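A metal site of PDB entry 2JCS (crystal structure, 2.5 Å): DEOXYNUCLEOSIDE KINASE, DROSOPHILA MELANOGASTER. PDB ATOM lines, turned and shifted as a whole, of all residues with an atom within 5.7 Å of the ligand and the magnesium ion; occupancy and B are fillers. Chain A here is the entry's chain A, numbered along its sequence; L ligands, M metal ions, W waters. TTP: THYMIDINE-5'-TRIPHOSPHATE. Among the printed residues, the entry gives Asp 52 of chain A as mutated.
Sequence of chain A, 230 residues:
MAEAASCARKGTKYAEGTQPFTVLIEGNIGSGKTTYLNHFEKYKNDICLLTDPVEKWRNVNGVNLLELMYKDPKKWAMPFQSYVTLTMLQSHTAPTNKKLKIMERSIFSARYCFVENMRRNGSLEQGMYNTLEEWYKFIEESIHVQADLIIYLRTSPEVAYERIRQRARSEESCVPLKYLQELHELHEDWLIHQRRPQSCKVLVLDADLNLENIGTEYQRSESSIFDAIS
The magnesium ion is bound by O1B of the ligand, O3G of the ligand, OG1 of Thr 34, water W2, OE2 of Glu 104 and OD1 of Asp 52.
The magnesium ion has six donor atoms within binding distance.
Of the 32 residues printed, 3 come within 4 Å of the magnesium ion.
Water W2 lies within hydrogen-bond range of the side-chain carboxylate of Asp 52 (3.1 Å), the guanidinium group of Arg 169 (3.2 Å) and the guanidinium group of Arg 167 (3.4 Å).
Water W3 lies within hydrogen-bond range of OH of Tyr 179 (2.6 Å), O2 of the ligand (2.7 Å) and OH of Tyr 70 (3.0 Å).
Water W4 lies within hydrogen-bond range of the side-chain hydroxyl of Thr 35 (2.9 Å) and the backbone NH of Thr 34 (3.1 Å).
The side-chain amide oxygen (OE1) of Gln 81 sits close to the side-chain sulfur (SD) of Met 118 (3.7 Å).
NH2 of Arg 105 is in hydrogen-bond range of O of Gly 27.
The backbone carbonyl oxygen (O) of Asn 28 is in hydrogen-bond range of the side-chain amino group (NZ) of Lys 33, at 2.8 Å.
The backbone carbonyl oxygen (O) of Gly 27 is in hydrogen-bond range of the side-chain amino group (NZ) of Lys 33.
The backbone carbonyl oxygen (O) of Asn 28 is in hydrogen-bond range of the side-chain hydroxyl (OG) of Ser 31 (2.9 Å).
The backbone NH (N) of Phe 114 sits at hydrogen-bond distance from the backbone carbonyl oxygen (O) of Ser 109, at 3.3 Å.
The backbone carbonyl oxygen (O) of Ala 110 sits at hydrogen-bond distance from the backbone NH (N) of Val 115.
O of Trp 57 sits at hydrogen-bond distance from N of Leu 66, at 3.4 Å.
O of Asn 28 touches O2G of the ligand, 3.7 Å away.
Ile 29 touches the ligand.
Val 54 touches the ligand.
Trp 57 touches the ligand.
Leu 66 touches the ligand (CD1 to O4', 3.4 Å).
Met 69 touches the ligand.
Phe 80 touches the ligand.
Val 84 touches the ligand.
CA of Ala 110 touches O4 of the ligand (3.3 Å).
CG of Phe 114 touches C4 of the ligand, 3.3 Å away.
Met 118 touches the ligand (CE to O2, 3.7 Å).
Hydrophobic or aromatic side chains that line the ligand: Ile 29, Val 54, Trp 57, Leu 66, Met 69, Tyr 70, Phe 80, Val 84, Ala 110, Phe 114 and Met 118.
The nearest printed residue that does not touch the ligand is Gly 27 (4.4 Å).
The backbone NH (N) of Thr 34 lies close to an oxygen (O3G) of the ligand, at 3.1 Å.
The side-chain hydroxyl of Tyr 70 lies within hydrogen-bond range of an oxygen (O3') of the ligand (2.6 Å).
O1G of the ligand is in salt-bridge range of NH1 of Arg 167 (2.6 Å).
N3 of the ligand is in hydrogen-bond range of OE1 of Gln 81 (2.7 Å).
O1A of the ligand is in salt-bridge range of NE of Arg 105, 2.8 Å away.
An oxygen (O2G) of the ligand lies within hydrogen-bond range of the backbone NH (N) of Lys 33 (2.8 Å).
The side-chain amino group (NZ) of Lys 33 lies within salt-bridge range of an oxygen (O2A) of the ligand (2.8 Å).
OE2 of Glu 172 lies within hydrogen-bond range of O3' of the ligand, at 2.9 Å.
The backbone NH (N) of Gly 32 sits at hydrogen-bond distance from an oxygen (O2G) of the ligand (3.0 Å).
The backbone NH (N) of Gly 30 sits at hydrogen-bond distance from an oxygen (O1G) of the ligand, at 3.1 Å.
The guanidinium group (NH1) of Arg 169 lies within salt-bridge range of an oxygen (O2B) of the ligand (3.1 Å).
The backbone NH (N) of Ser 31 sits at hydrogen-bond distance from an oxygen (O2G) of the ligand (3.2 Å).
OG of Ser 31 is in hydrogen-bond range of O2G of the ligand.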
ATOM      1  N   GLY A  27      26.707  14.343  18.891  1.00  0.00           N
ATOM      2  CA  GLY A  27      26.224  12.972  19.004  1.00  0.00           C
ATOM      3  C   GLY A  27      25.524  12.560  17.731  1.00  0.00           C
ATOM      4  O   GLY A  27      25.198  13.401  16.895  1.00  0.00           O
ATOM      5  N   ASN A  28      25.286  11.260  17.600  1.00  0.00           N
ATOM      6  CA  ASN A  28      24.643  10.681  16.412  1.00  0.00           C
ATOM      7  C   ASN A  28      23.238  11.228  16.138  1.00  0.00           C
ATOM      8  O   ASN A  28      22.663  11.913  16.983  1.00  0.00           O
ATOM      9  CB  ASN A  28      24.589   9.159  16.558  1.00  0.00           C
ATOM     10  CG  ASN A  28      24.896   8.442  15.268  1.00  0.00           C
ATOM     11  OD1 ASN A  28      24.599   8.928  14.170  1.00  0.00           O
ATOM     12  ND2 ASN A  28      25.503   7.264  15.380  1.00  0.00           N
ATOM     13  N   ILE A  29      22.698  10.932  14.965  1.00  0.00           N
ATOM     14  CA  ILE A  29      21.308  11.234  14.665  1.00  0.00           C
ATOM     15  C   ILE A  29      20.438  10.453  15.636  1.00  0.00           C
ATOM     16  O   ILE A  29      20.600   9.245  15.779  1.00  0.00           O
ATOM     17  CB  ILE A  29      20.926  10.856  13.208  1.00  0.00           C
ATOM     18  CG1 ILE A  29      21.995  11.312  12.208  1.00  0.00           C
ATOM     19  CG2 ILE A  29      19.557  11.439  12.844  1.00  0.00           C
ATOM     20  CD1 ILE A  29      22.034  10.474  10.948  1.00  0.00           C
ATOM     21  N   GLY A  30      19.532  11.158  16.314  1.00  0.00           N
ATOM     22  CA  GLY A  30      18.661  10.537  17.303  1.00  0.00           C
ATOM     23  C   GLY A  30      19.379  10.172  18.586  1.00  0.00           C
ATOM     24  O   GLY A  30      19.066   9.152  19.202  1.00  0.00           O
ATOM     25  N   SER A  31      20.350  11.005  18.983  1.00  0.00           N
ATOM     26  CA  SER A  31      21.070  10.809  20.240  1.00  0.00           C
ATOM     27  C   SER A  31      20.445  11.642  21.362  1.00  0.00           C
ATOM     28  O   SER A  31      20.803  11.488  22.525  1.00  0.00           O
ATOM     29  CB  SER A  31      22.560  11.134  20.090  1.00  0.00           C
ATOM     30  OG  SER A  31      22.762  12.513  19.842  1.00  0.00           O
ATOM     31  N   GLY A  32      19.509  12.507  20.986  1.00  0.00           N
ATOM     32  CA  GLY A  32      18.803  13.351  21.937  1.00  0.00           C
ATOM     33  C   GLY A  32      19.447  14.703  22.146  1.00  0.00           C
ATOM     34  O   GLY A  32      19.449  15.224  23.269  1.00  0.00           O
ATOM     35  N   LYS A  33      20.002  15.276  21.073  1.00  0.00           N
ATOM     36  CA  LYS A  33      20.641  16.585  21.143  1.00  0.00           C
ATOM     37  C   LYS A  33      19.641  17.688  21.460  1.00  0.00           C
ATOM     38  O   LYS A  33      19.908  18.535  22.318  1.00  0.00           O
ATOM     39  CB  LYS A  33      21.388  16.884  19.832  1.00  0.00           C
ATOM     40  CG  LYS A  33      22.665  16.071  19.629  1.00  0.00           C
ATOM     41  CD  LYS A  33      23.478  16.571  18.426  1.00  0.00           C
ATOM     42  CE  LYS A  33      22.864  16.159  17.090  1.00  0.00           C
ATOM     43  NZ  LYS A  33      22.522  14.708  17.005  1.00  0.00           N
ATOM     44  N   THR A  34      18.503  17.672  20.777  1.00  0.00           N
ATOM     45  CA  THR A  34      17.440  18.653  20.994  1.00  0.00           C
ATOM     46  C   THR A  34      16.766  18.476  22.369  1.00  0.00           C
ATOM     47  O   THR A  34      16.482  19.462  23.055  1.00  0.00           O
ATOM     48  CB  THR A  34      16.385  18.598  19.867  1.00  0.00           C
ATOM     49  OG1 THR A  34      17.044  18.573  18.592  1.00  0.00           O
ATOM     50  CG2 THR A  34      15.573  19.878  19.807  1.00  0.00           C
ATOM     51  N   THR A  35      16.530  17.222  22.753  1.00  0.00           N
ATOM     52  CA  THR A  35      15.941  16.903  24.060  1.00  0.00           C
ATOM     53  C   THR A  35      16.786  17.422  25.214  1.00  0.00           C
ATOM     54  O   THR A  35      16.257  17.936  26.202  1.00  0.00           O
ATOM     55  CB  THR A  35      15.738  15.372  24.205  1.00  0.00           C
ATOM     56  OG1 THR A  35      15.164  14.846  23.001  1.00  0.00           O
ATOM     57  CG2 THR A  35      14.671  15.078  25.250  1.00  0.00           C
ATOM     58  N   ASP A  52      18.142  22.498  16.743  1.00  0.00           N
ATOM     59  CA  ASP A  52      17.596  21.917  15.519  1.00  0.00           C
ATOM     60  C   ASP A  52      17.801  22.751  14.249  1.00  0.00           C
ATOM     61  O   ASP A  52      16.843  23.285  13.692  1.00  0.00           O
ATOM     62  CB  ASP A  52      16.113  21.577  15.712  1.00  0.00           C
ATOM     63  CG  ASP A  52      15.875  20.100  15.977  1.00  0.00           C
ATOM     64  OD1 ASP A  52      16.851  19.313  15.946  1.00  0.00           O
ATOM     65  OD2 ASP A  52      14.748  19.620  16.215  1.00  0.00           O
ATOM     66  N   VAL A  54      18.486  21.411  11.529  1.00  0.00           N
ATOM     67  CA  VAL A  54      17.892  20.545  10.514  1.00  0.00           C
ATOM     68  C   VAL A  54      16.618  21.124   9.865  1.00  0.00           C
ATOM     69  O   VAL A  54      16.324  20.831   8.707  1.00  0.00           O
ATOM     70  CB  VAL A  54      17.637  19.098  11.055  1.00  0.00           C
ATOM     71  CG1 VAL A  54      16.524  19.077  12.113  1.00  0.00           C
ATOM     72  CG2 VAL A  54      17.323  18.134   9.924  1.00  0.00           C
ATOM     73  N   TRP A  57      17.433  23.037   6.849  1.00  0.00           N
ATOM     74  CA  TRP A  57      17.795  22.164   5.729  1.00  0.00           C
ATOM     75  C   TRP A  57      16.583  21.503   5.076  1.00  0.00           C
ATOM     76  O   TRP A  57      16.611  21.143   3.905  1.00  0.00           O
ATOM     77  CB  TRP A  57      18.816  21.100   6.162  1.00  0.00           C
ATOM     78  CG  TRP A  57      19.900  21.607   7.084  1.00  0.00           C
ATOM     79  CD1 TRP A  57      20.453  22.857   7.109  1.00  0.00           C
ATOM     80  CD2 TRP A  57      20.569  20.861   8.114  1.00  0.00           C
ATOM     81  NE1 TRP A  57      21.413  22.935   8.093  1.00  0.00           N
ATOM     82  CE2 TRP A  57      21.502  21.735   8.724  1.00  0.00           C
ATOM     83  CE3 TRP A  57      20.472  19.543   8.584  1.00  0.00           C
ATOM     84  CZ2 TRP A  57      22.332  21.324   9.774  1.00  0.00           C
ATOM     85  CZ3 TRP A  57      21.287  19.147   9.641  1.00  0.00           C
ATOM     86  CH2 TRP A  57      22.203  20.034  10.216  1.00  0.00           C
ATOM     87  N   LEU A  66      17.213  18.117   2.596  1.00  0.00           N
ATOM     88  CA  LEU A  66      17.398  16.852   3.324  1.00  0.00           C
ATOM     89  C   LEU A  66      16.777  15.672   2.567  1.00  0.00           C
ATOM     90  O   LEU A  66      17.417  14.633   2.432  1.00  0.00           O
ATOM     91  CB  LEU A  66      16.835  16.949   4.749  1.00  0.00           C
ATOM     92  CG  LEU A  66      17.112  15.783   5.711  1.00  0.00           C
ATOM     93  CD1 LEU A  66      18.563  15.756   6.200  1.00  0.00           C
ATOM     94  CD2 LEU A  66      16.164  15.841   6.907  1.00  0.00           C
ATOM     95  N   MET A  69      18.738  14.992  -0.687  1.00  0.00           N
ATOM     96  CA  MET A  69      20.007  14.341  -0.366  1.00  0.00           C
ATOM     97  C   MET A  69      19.821  12.840  -0.168  1.00  0.00           C
ATOM     98  O   MET A  69      20.603  12.045  -0.695  1.00  0.00           O
ATOM     99  CB  MET A  69      20.648  14.981   0.867  1.00  0.00           C
ATOM    100  CG  MET A  69      22.032  14.430   1.235  1.00  0.00           C
ATOM    101  SD  MET A  69      21.961  12.885   2.188  1.00  0.00           S
ATOM    102  CE  MET A  69      21.490  13.504   3.818  1.00  0.00           C
ATOM    103  N   TYR A  70      18.797  12.455   0.588  1.00  0.00           N
ATOM    104  CA  TYR A  70      18.527  11.049   0.872  1.00  0.00           C
ATOM    105  C   TYR A  70      17.999  10.294  -0.348  1.00  0.00           C
ATOM    106  O   TYR A  70      18.299   9.105  -0.524  1.00  0.00           O
ATOM    107  CB  TYR A  70      17.578  10.895   2.062  1.00  0.00           C
ATOM    108  CG  TYR A  70      18.247  11.000   3.415  1.00  0.00           C
ATOM    109  CD1 TYR A  70      17.846  11.973   4.340  1.00  0.00           C
ATOM    110  CD2 TYR A  70      19.285  10.141   3.776  1.00  0.00           C
ATOM    111  CE1 TYR A  70      18.455  12.079   5.585  1.00  0.00           C
ATOM    112  CE2 TYR A  70      19.905  10.249   5.012  1.00  0.00           C
ATOM    113  CZ  TYR A  70      19.486  11.211   5.911  1.00  0.00           C
ATOM    114  OH  TYR A  70      20.100  11.306   7.149  1.00  0.00           O
ATOM    115  N   PHE A  80      23.834  19.929  -0.426  1.00  0.00           N
ATOM    116  CA  PHE A  80      23.276  19.811   0.915  1.00  0.00           C
ATOM    117  C   PHE A  80      24.315  20.067   2.008  1.00  0.00           C
ATOM    118  O   PHE A  80      24.059  20.809   2.958  1.00  0.00           O
ATOM    119  CB  PHE A  80      22.608  18.436   1.121  1.00  0.00           C
ATOM    120  CG  PHE A  80      22.227  18.149   2.545  1.00  0.00           C
ATOM    121  CD1 PHE A  80      21.067  18.685   3.091  1.00  0.00           C
ATOM    122  CD2 PHE A  80      23.043  17.363   3.345  1.00  0.00           C
ATOM    123  CE1 PHE A  80      20.718  18.427   4.418  1.00  0.00           C
ATOM    124  CE2 PHE A  80      22.715  17.102   4.662  1.00  0.00           C
ATOM    125  CZ  PHE A  80      21.542  17.636   5.203  1.00  0.00           C
ATOM    126  N   GLN A  81      25.483  19.438   1.872  1.00  0.00           N
ATOM    127  CA  GLN A  81      26.563  19.630   2.838  1.00  0.00           C
ATOM    128  C   GLN A  81      27.100  21.061   2.801  1.00  0.00           C
ATOM    129  O   GLN A  81      27.453  21.627   3.836  1.00  0.00           O
ATOM    130  CB  GLN A  81      27.690  18.619   2.619  1.00  0.00           C
ATOM    131  CG  GLN A  81      27.393  17.203   3.133  1.00  0.00           C
ATOM    132  CD  GLN A  81      26.941  17.158   4.588  1.00  0.00           C
ATOM    133  OE1 GLN A  81      26.039  16.395   4.927  1.00  0.00           O
ATOM    134  NE2 GLN A  81      27.574  17.957   5.448  1.00  0.00           N
ATOM    135  N   VAL A  84      24.560  22.931   4.795  1.00  0.00           N
ATOM    136  CA  VAL A  84      24.762  22.588   6.204  1.00  0.00           C
ATOM    137  C   VAL A  84      25.899  23.426   6.786  1.00  0.00           C
ATOM    138  O   VAL A  84      25.742  24.038   7.837  1.00  0.00           O
ATOM    139  CB  VAL A  84      25.033  21.067   6.402  1.00  0.00           C
ATOM    140  CG1 VAL A  84      25.565  20.787   7.808  1.00  0.00           C
ATOM    141  CG2 VAL A  84      23.767  20.273   6.176  1.00  0.00           C
ATOM    142  N   GLU A 104      23.310  23.175  19.045  1.00  0.00           N
ATOM    143  CA  GLU A 104      23.130  21.828  18.521  1.00  0.00           C
ATOM    144  C   GLU A 104      23.949  21.719  17.232  1.00  0.00           C
ATOM    145  O   GLU A 104      23.764  22.515  16.302  1.00  0.00           O
ATOM    146  CB  GLU A 104      21.660  21.541  18.240  1.00  0.00           C
ATOM    147  CG  GLU A 104      21.384  20.189  17.603  1.00  0.00           C
ATOM    148  CD  GLU A 104      19.940  19.753  17.735  1.00  0.00           C
ATOM    149  OE1 GLU A 104      19.112  20.518  18.289  1.00  0.00           O
ATOM    150  OE2 GLU A 104      19.627  18.628  17.299  1.00  0.00           O
ATOM    151  N   ARG A 105      24.860  20.751  17.198  1.00  0.00           N
ATOM    152  CA  ARG A 105      25.754  20.505  16.062  1.00  0.00           C
ATOM    153  C   ARG A 105      26.774  21.618  15.845  1.00  0.00           C
ATOM    154  O   ARG A 105      26.734  22.653  16.515  1.00  0.00           O
ATOM    155  CB  ARG A 105      24.950  20.226  14.767  1.00  0.00           C
ATOM    156  CG  ARG A 105      24.363  18.820  14.678  1.00  0.00           C
ATOM    157  CD  ARG A 105      25.387  17.744  14.350  1.00  0.00           C
ATOM    158  NE  ARG A 105      24.763  16.431  14.165  1.00  0.00           N
ATOM    159  CZ  ARG A 105      25.346  15.276  14.455  1.00  0.00           C
ATOM    160  NH1 ARG A 105      26.574  15.245  14.949  1.00  0.00           N
ATOM    161  NH2 ARG A 105      24.694  14.140  14.253  1.00  0.00           N
ATOM    162  N   SER A 106      27.699  21.395  14.904  1.00  0.00           N
ATOM    163  CA  SER A 106      28.729  22.356  14.562  1.00  0.00           C
ATOM    164  C   SER A 106      29.305  22.075  13.170  1.00  0.00           C
ATOM    165  O   SER A 106      29.007  21.044  12.576  1.00  0.00           O
ATOM    166  CB  SER A 106      29.861  22.326  15.596  1.00  0.00           C
ATOM    167  OG  SER A 106      30.490  21.059  15.634  1.00  0.00           O
ATOM    168  N   SER A 109      31.396  18.607  13.109  1.00  0.00           N
ATOM    169  CA  SER A 109      30.710  17.329  12.905  1.00  0.00           C
ATOM    170  C   SER A 109      30.276  17.143  11.459  1.00  0.00           C
ATOM    171  O   SER A 109      30.312  16.039  10.929  1.00  0.00           O
ATOM    172  CB  SER A 109      29.518  17.177  13.851  1.00  0.00           C
ATOM    173  OG  SER A 109      28.593  18.231  13.674  1.00  0.00           O
ATOM    174  N   ALA A 110      29.859  18.238  10.826  1.00  0.00           N
ATOM    175  CA  ALA A 110      29.500  18.231   9.412  1.00  0.00           C
ATOM    176  C   ALA A 110      30.682  17.770   8.567  1.00  0.00           C
ATOM    177  O   ALA A 110      30.533  16.919   7.678  1.00  0.00           O
ATOM    178  CB  ALA A 110      29.015  19.606   8.971  1.00  0.00           C
ATOM    179  N   ARG A 111      31.862  18.306   8.868  1.00  0.00           N
ATOM    180  CA  ARG A 111      33.095  17.962   8.167  1.00  0.00           C
ATOM    181  C   ARG A 111      33.594  16.556   8.524  1.00  0.00           C
ATOM    182  O   ARG A 111      33.671  15.687   7.654  1.00  0.00           O
ATOM    183  CB  ARG A 111      34.184  19.006   8.475  1.00  0.00           C
ATOM    184  CG  ARG A 111      35.540  18.701   7.868  1.00  0.00           C
ATOM    185  CD  ARG A 111      36.602  19.729   8.208  1.00  0.00           C
ATOM    186  NE  ARG A 111      37.745  19.634   7.305  1.00  0.00           N
ATOM    187  CZ  ARG A 111      38.859  20.355   7.428  1.00  0.00           C
ATOM    188  NH1 ARG A 111      38.998  21.221   8.416  1.00  0.00           N
ATOM    189  NH2 ARG A 111      39.844  20.204   6.548  1.00  0.00           N
ATOM    190  N   PHE A 114      30.042  13.621   8.745  1.00  0.00           N
ATOM    191  CA  PHE A 114      29.102  13.458   7.638  1.00  0.00           C
ATOM    192  C   PHE A 114      29.729  13.561   6.243  1.00  0.00           C
ATOM    193  O   PHE A 114      29.483  12.713   5.390  1.00  0.00           O
ATOM    194  CB  PHE A 114      27.918  14.425   7.779  1.00  0.00           C
ATOM    195  CG  PHE A 114      26.983  14.052   8.898  1.00  0.00           C
ATOM    196  CD1 PHE A 114      27.169  14.573  10.169  1.00  0.00           C
ATOM    197  CD2 PHE A 114      25.923  13.177   8.674  1.00  0.00           C
ATOM    198  CE1 PHE A 114      26.310  14.226  11.201  1.00  0.00           C
ATOM    199  CE2 PHE A 114      25.063  12.830   9.707  1.00  0.00           C
ATOM    200  CZ  PHE A 114      25.261  13.353  10.970  1.00  0.00           C
ATOM    201  N   VAL A 115      30.527  14.606   6.020  1.00  0.00           N
ATOM    202  CA  VAL A 115      31.234  14.772   4.750  1.00  0.00           C
ATOM    203  C   VAL A 115      32.193  13.596   4.534  1.00  0.00           C
ATOM    204  O   VAL A 115      32.250  13.035   3.438  1.00  0.00           O
ATOM    205  CB  VAL A 115      31.969  16.135   4.659  1.00  0.00           C
ATOM    206  CG1 VAL A 115      32.984  16.169   3.515  1.00  0.00           C
ATOM    207  CG2 VAL A 115      30.960  17.269   4.490  1.00  0.00           C
ATOM    208  N   MET A 118      30.247  10.369   3.679  1.00  0.00           N
ATOM    209  CA  MET A 118      29.701  10.497   2.335  1.00  0.00           C
ATOM    210  C   MET A 118      30.797  10.344   1.269  1.00  0.00           C
ATOM    211  O   MET A 118      30.519   9.967   0.130  1.00  0.00           O
ATOM    212  CB  MET A 118      28.975  11.828   2.172  1.00  0.00           C
ATOM    213  CG  MET A 118      27.549  11.833   2.685  1.00  0.00           C
ATOM    214  SD  MET A 118      26.914  13.505   2.875  1.00  0.00           S
ATOM    215  CE  MET A 118      25.429  13.202   3.834  1.00  0.00           C
ATOM    216  N   ARG A 167      10.550   9.414  16.115  1.00  0.00           N
ATOM    217  CA  ARG A 167      10.380  10.763  15.572  1.00  0.00           C
ATOM    218  C   ARG A 167       9.672  10.714  14.211  1.00  0.00           C
ATOM    219  O   ARG A 167       8.801  11.543  13.931  1.00  0.00           O
ATOM    220  CB  ARG A 167      11.733  11.471  15.463  1.00  0.00           C
ATOM    221  CG  ARG A 167      11.678  12.894  14.935  1.00  0.00           C
ATOM    222  CD  ARG A 167      13.003  13.639  15.039  1.00  0.00           C
ATOM    223  NE  ARG A 167      14.107  12.901  14.411  1.00  0.00           N
ATOM    224  CZ  ARG A 167      15.333  12.817  14.916  1.00  0.00           C
ATOM    225  NH1 ARG A 167      15.636  13.432  16.050  1.00  0.00           N
ATOM    226  NH2 ARG A 167      16.260  12.128  14.270  1.00  0.00           N
ATOM    227  N   ARG A 169      10.614  11.226  10.920  1.00  0.00           N
ATOM    228  CA  ARG A 169      10.861  12.154   9.826  1.00  0.00           C
ATOM    229  C   ARG A 169      10.803  11.372   8.512  1.00  0.00           C
ATOM    230  O   ARG A 169      11.555  10.409   8.341  1.00  0.00           O
ATOM    231  CB  ARG A 169      12.234  12.810   9.968  1.00  0.00           C
ATOM    232  CG  ARG A 169      12.354  13.883  11.042  1.00  0.00           C
ATOM    233  CD  ARG A 169      13.636  14.698  10.953  1.00  0.00           C
ATOM    234  NE  ARG A 169      13.902  15.458  12.172  1.00  0.00           N
ATOM    235  CZ  ARG A 169      15.076  15.536  12.783  1.00  0.00           C
ATOM    236  NH1 ARG A 169      16.126  14.878  12.304  1.00  0.00           N
ATOM    237  NH2 ARG A 169      15.205  16.254  13.889  1.00  0.00           N
ATOM    238  N   GLU A 172      14.035  10.554   6.773  1.00  0.00           N
ATOM    239  CA  GLU A 172      14.931   9.623   7.449  1.00  0.00           C
ATOM    240  C   GLU A 172      14.404   8.188   7.499  1.00  0.00           C
ATOM    241  O   GLU A 172      14.962   7.338   8.182  1.00  0.00           O
ATOM    242  CB  GLU A 172      15.237  10.126   8.861  1.00  0.00           C
ATOM    243  CG  GLU A 172      16.122  11.371   8.908  1.00  0.00           C
ATOM    244  CD  GLU A 172      16.194  12.012  10.287  1.00  0.00           C
ATOM    245  OE1 GLU A 172      15.666  11.438  11.252  1.00  0.00           O
ATOM    246  OE2 GLU A 172      16.801  13.088  10.391  1.00  0.00           O
ATOM    247  N   VAL A 175      16.924   5.341   6.272  1.00  0.00           N
ATOM    248  CA  VAL A 175      18.251   5.317   6.892  1.00  0.00           C
ATOM    249  C   VAL A 175      18.508   3.955   7.556  1.00  0.00           C
ATOM    250  O   VAL A 175      17.811   3.585   8.506  1.00  0.00           O
ATOM    251  CB  VAL A 175      18.424   6.461   7.921  1.00  0.00           C
ATOM    252  CG1 VAL A 175      19.767   6.346   8.646  1.00  0.00           C
ATOM    253  CG2 VAL A 175      18.304   7.811   7.239  1.00  0.00           C
ATOM    254  N   TYR A 179      24.482   2.717   8.242  1.00  0.00           N
ATOM    255  CA  TYR A 179      24.797   4.153   8.152  1.00  0.00           C
ATOM    256  C   TYR A 179      25.084   4.756   9.530  1.00  0.00           C
ATOM    257  O   TYR A 179      26.054   5.495   9.699  1.00  0.00           O
ATOM    258  CB  TYR A 179      23.654   4.893   7.460  1.00  0.00           C
ATOM    259  CG  TYR A 179      23.943   6.327   7.087  1.00  0.00           C
ATOM    260  CD1 TYR A 179      25.003   6.655   6.246  1.00  0.00           C
ATOM    261  CD2 TYR A 179      23.143   7.369   7.563  1.00  0.00           C
ATOM    262  CE1 TYR A 179      25.272   7.975   5.898  1.00  0.00           C
ATOM    263  CE2 TYR A 179      23.392   8.692   7.222  1.00  0.00           C
ATOM    264  CZ  TYR A 179      24.470   8.989   6.389  1.00  0.00           C
ATOM    265  OH  TYR A 179      24.732  10.290   6.050  1.00  0.00           O
HETATM  266  PA  TTP L   1      21.366  15.711  13.387  1.00  0.00           P
HETATM  267  O1A TTP L   1      22.283  16.817  12.938  1.00  0.00           O
HETATM  268  O2A TTP L   1      21.903  14.591  14.233  1.00  0.00           O
HETATM  269  O3A TTP L   1      20.116  16.412  14.122  1.00  0.00           O
HETATM  270  PB  TTP L   1      18.982  15.606  14.938  1.00  0.00           P
HETATM  271  O1B TTP L   1      17.929  16.615  15.308  1.00  0.00           O
HETATM  272  O2B TTP L   1      18.570  14.379  14.147  1.00  0.00           O
HETATM  273  O3B TTP L   1      19.770  15.125  16.259  1.00  0.00           O
HETATM  274  PG  TTP L   1      19.021  14.700  17.630  1.00  0.00           P
HETATM  275  O1G TTP L   1      18.007  13.662  17.194  1.00  0.00           O
HETATM  276  O2G TTP L   1      20.125  14.139  18.497  1.00  0.00           O
HETATM  277  O3G TTP L   1      18.410  15.971  18.145  1.00  0.00           O
HETATM  278  O5' TTP L   1      20.710  15.047  12.079  1.00  0.00           O
HETATM  279  C5' TTP L   1      19.780  15.759  11.265  1.00  0.00           C
HETATM  280  C4' TTP L   1      19.700  15.150   9.856  1.00  0.00           C
HETATM  281  O4' TTP L   1      20.575  15.861   8.989  1.00  0.00           O
HETATM  282  C3' TTP L   1      20.120  13.688   9.796  1.00  0.00           C
HETATM  283  O3' TTP L   1      19.246  13.015   8.904  1.00  0.00           O
HETATM  284  C2' TTP L   1      21.519  13.680   9.208  1.00  0.00           C
HETATM  285  C1' TTP L   1      21.576  14.991   8.436  1.00  0.00           C
HETATM  286  N1  TTP L   1      22.882  15.654   8.498  1.00  0.00           N
HETATM  287  C2  TTP L   1      23.712  15.547   7.421  1.00  0.00           C
HETATM  288  O2  TTP L   1      23.353  14.871   6.431  1.00  0.00           O
HETATM  289  N3  TTP L   1      24.911  16.157   7.396  1.00  0.00           N
HETATM  290  C4  TTP L   1      25.337  16.877   8.442  1.00  0.00           C
HETATM  291  O4  TTP L   1      26.454  17.431   8.412  1.00  0.00           O
HETATM  292  C5  TTP L   1      24.450  17.016   9.627  1.00  0.00           C
HETATM  293  C5M TTP L   1      24.859  17.824  10.825  1.00  0.00           C
HETATM  294  C6  TTP L   1      23.218  16.367   9.587  1.00  0.00           C
HETATM  295 MG    MG M   1      17.687  17.362  16.954  1.00  0.00          MG
HETATM  296  O   HOH W   1      19.899  19.140  13.913  1.00  0.00           O
HETATM  297  O   HOH W   2      15.596  16.742  16.988  1.00  0.00           O
HETATM  298  O   HOH W   3      22.955  12.169   6.517  1.00  0.00           O
HETATM  299  O   HOH W   4      16.526  15.299  20.498  1.00  0.00           O
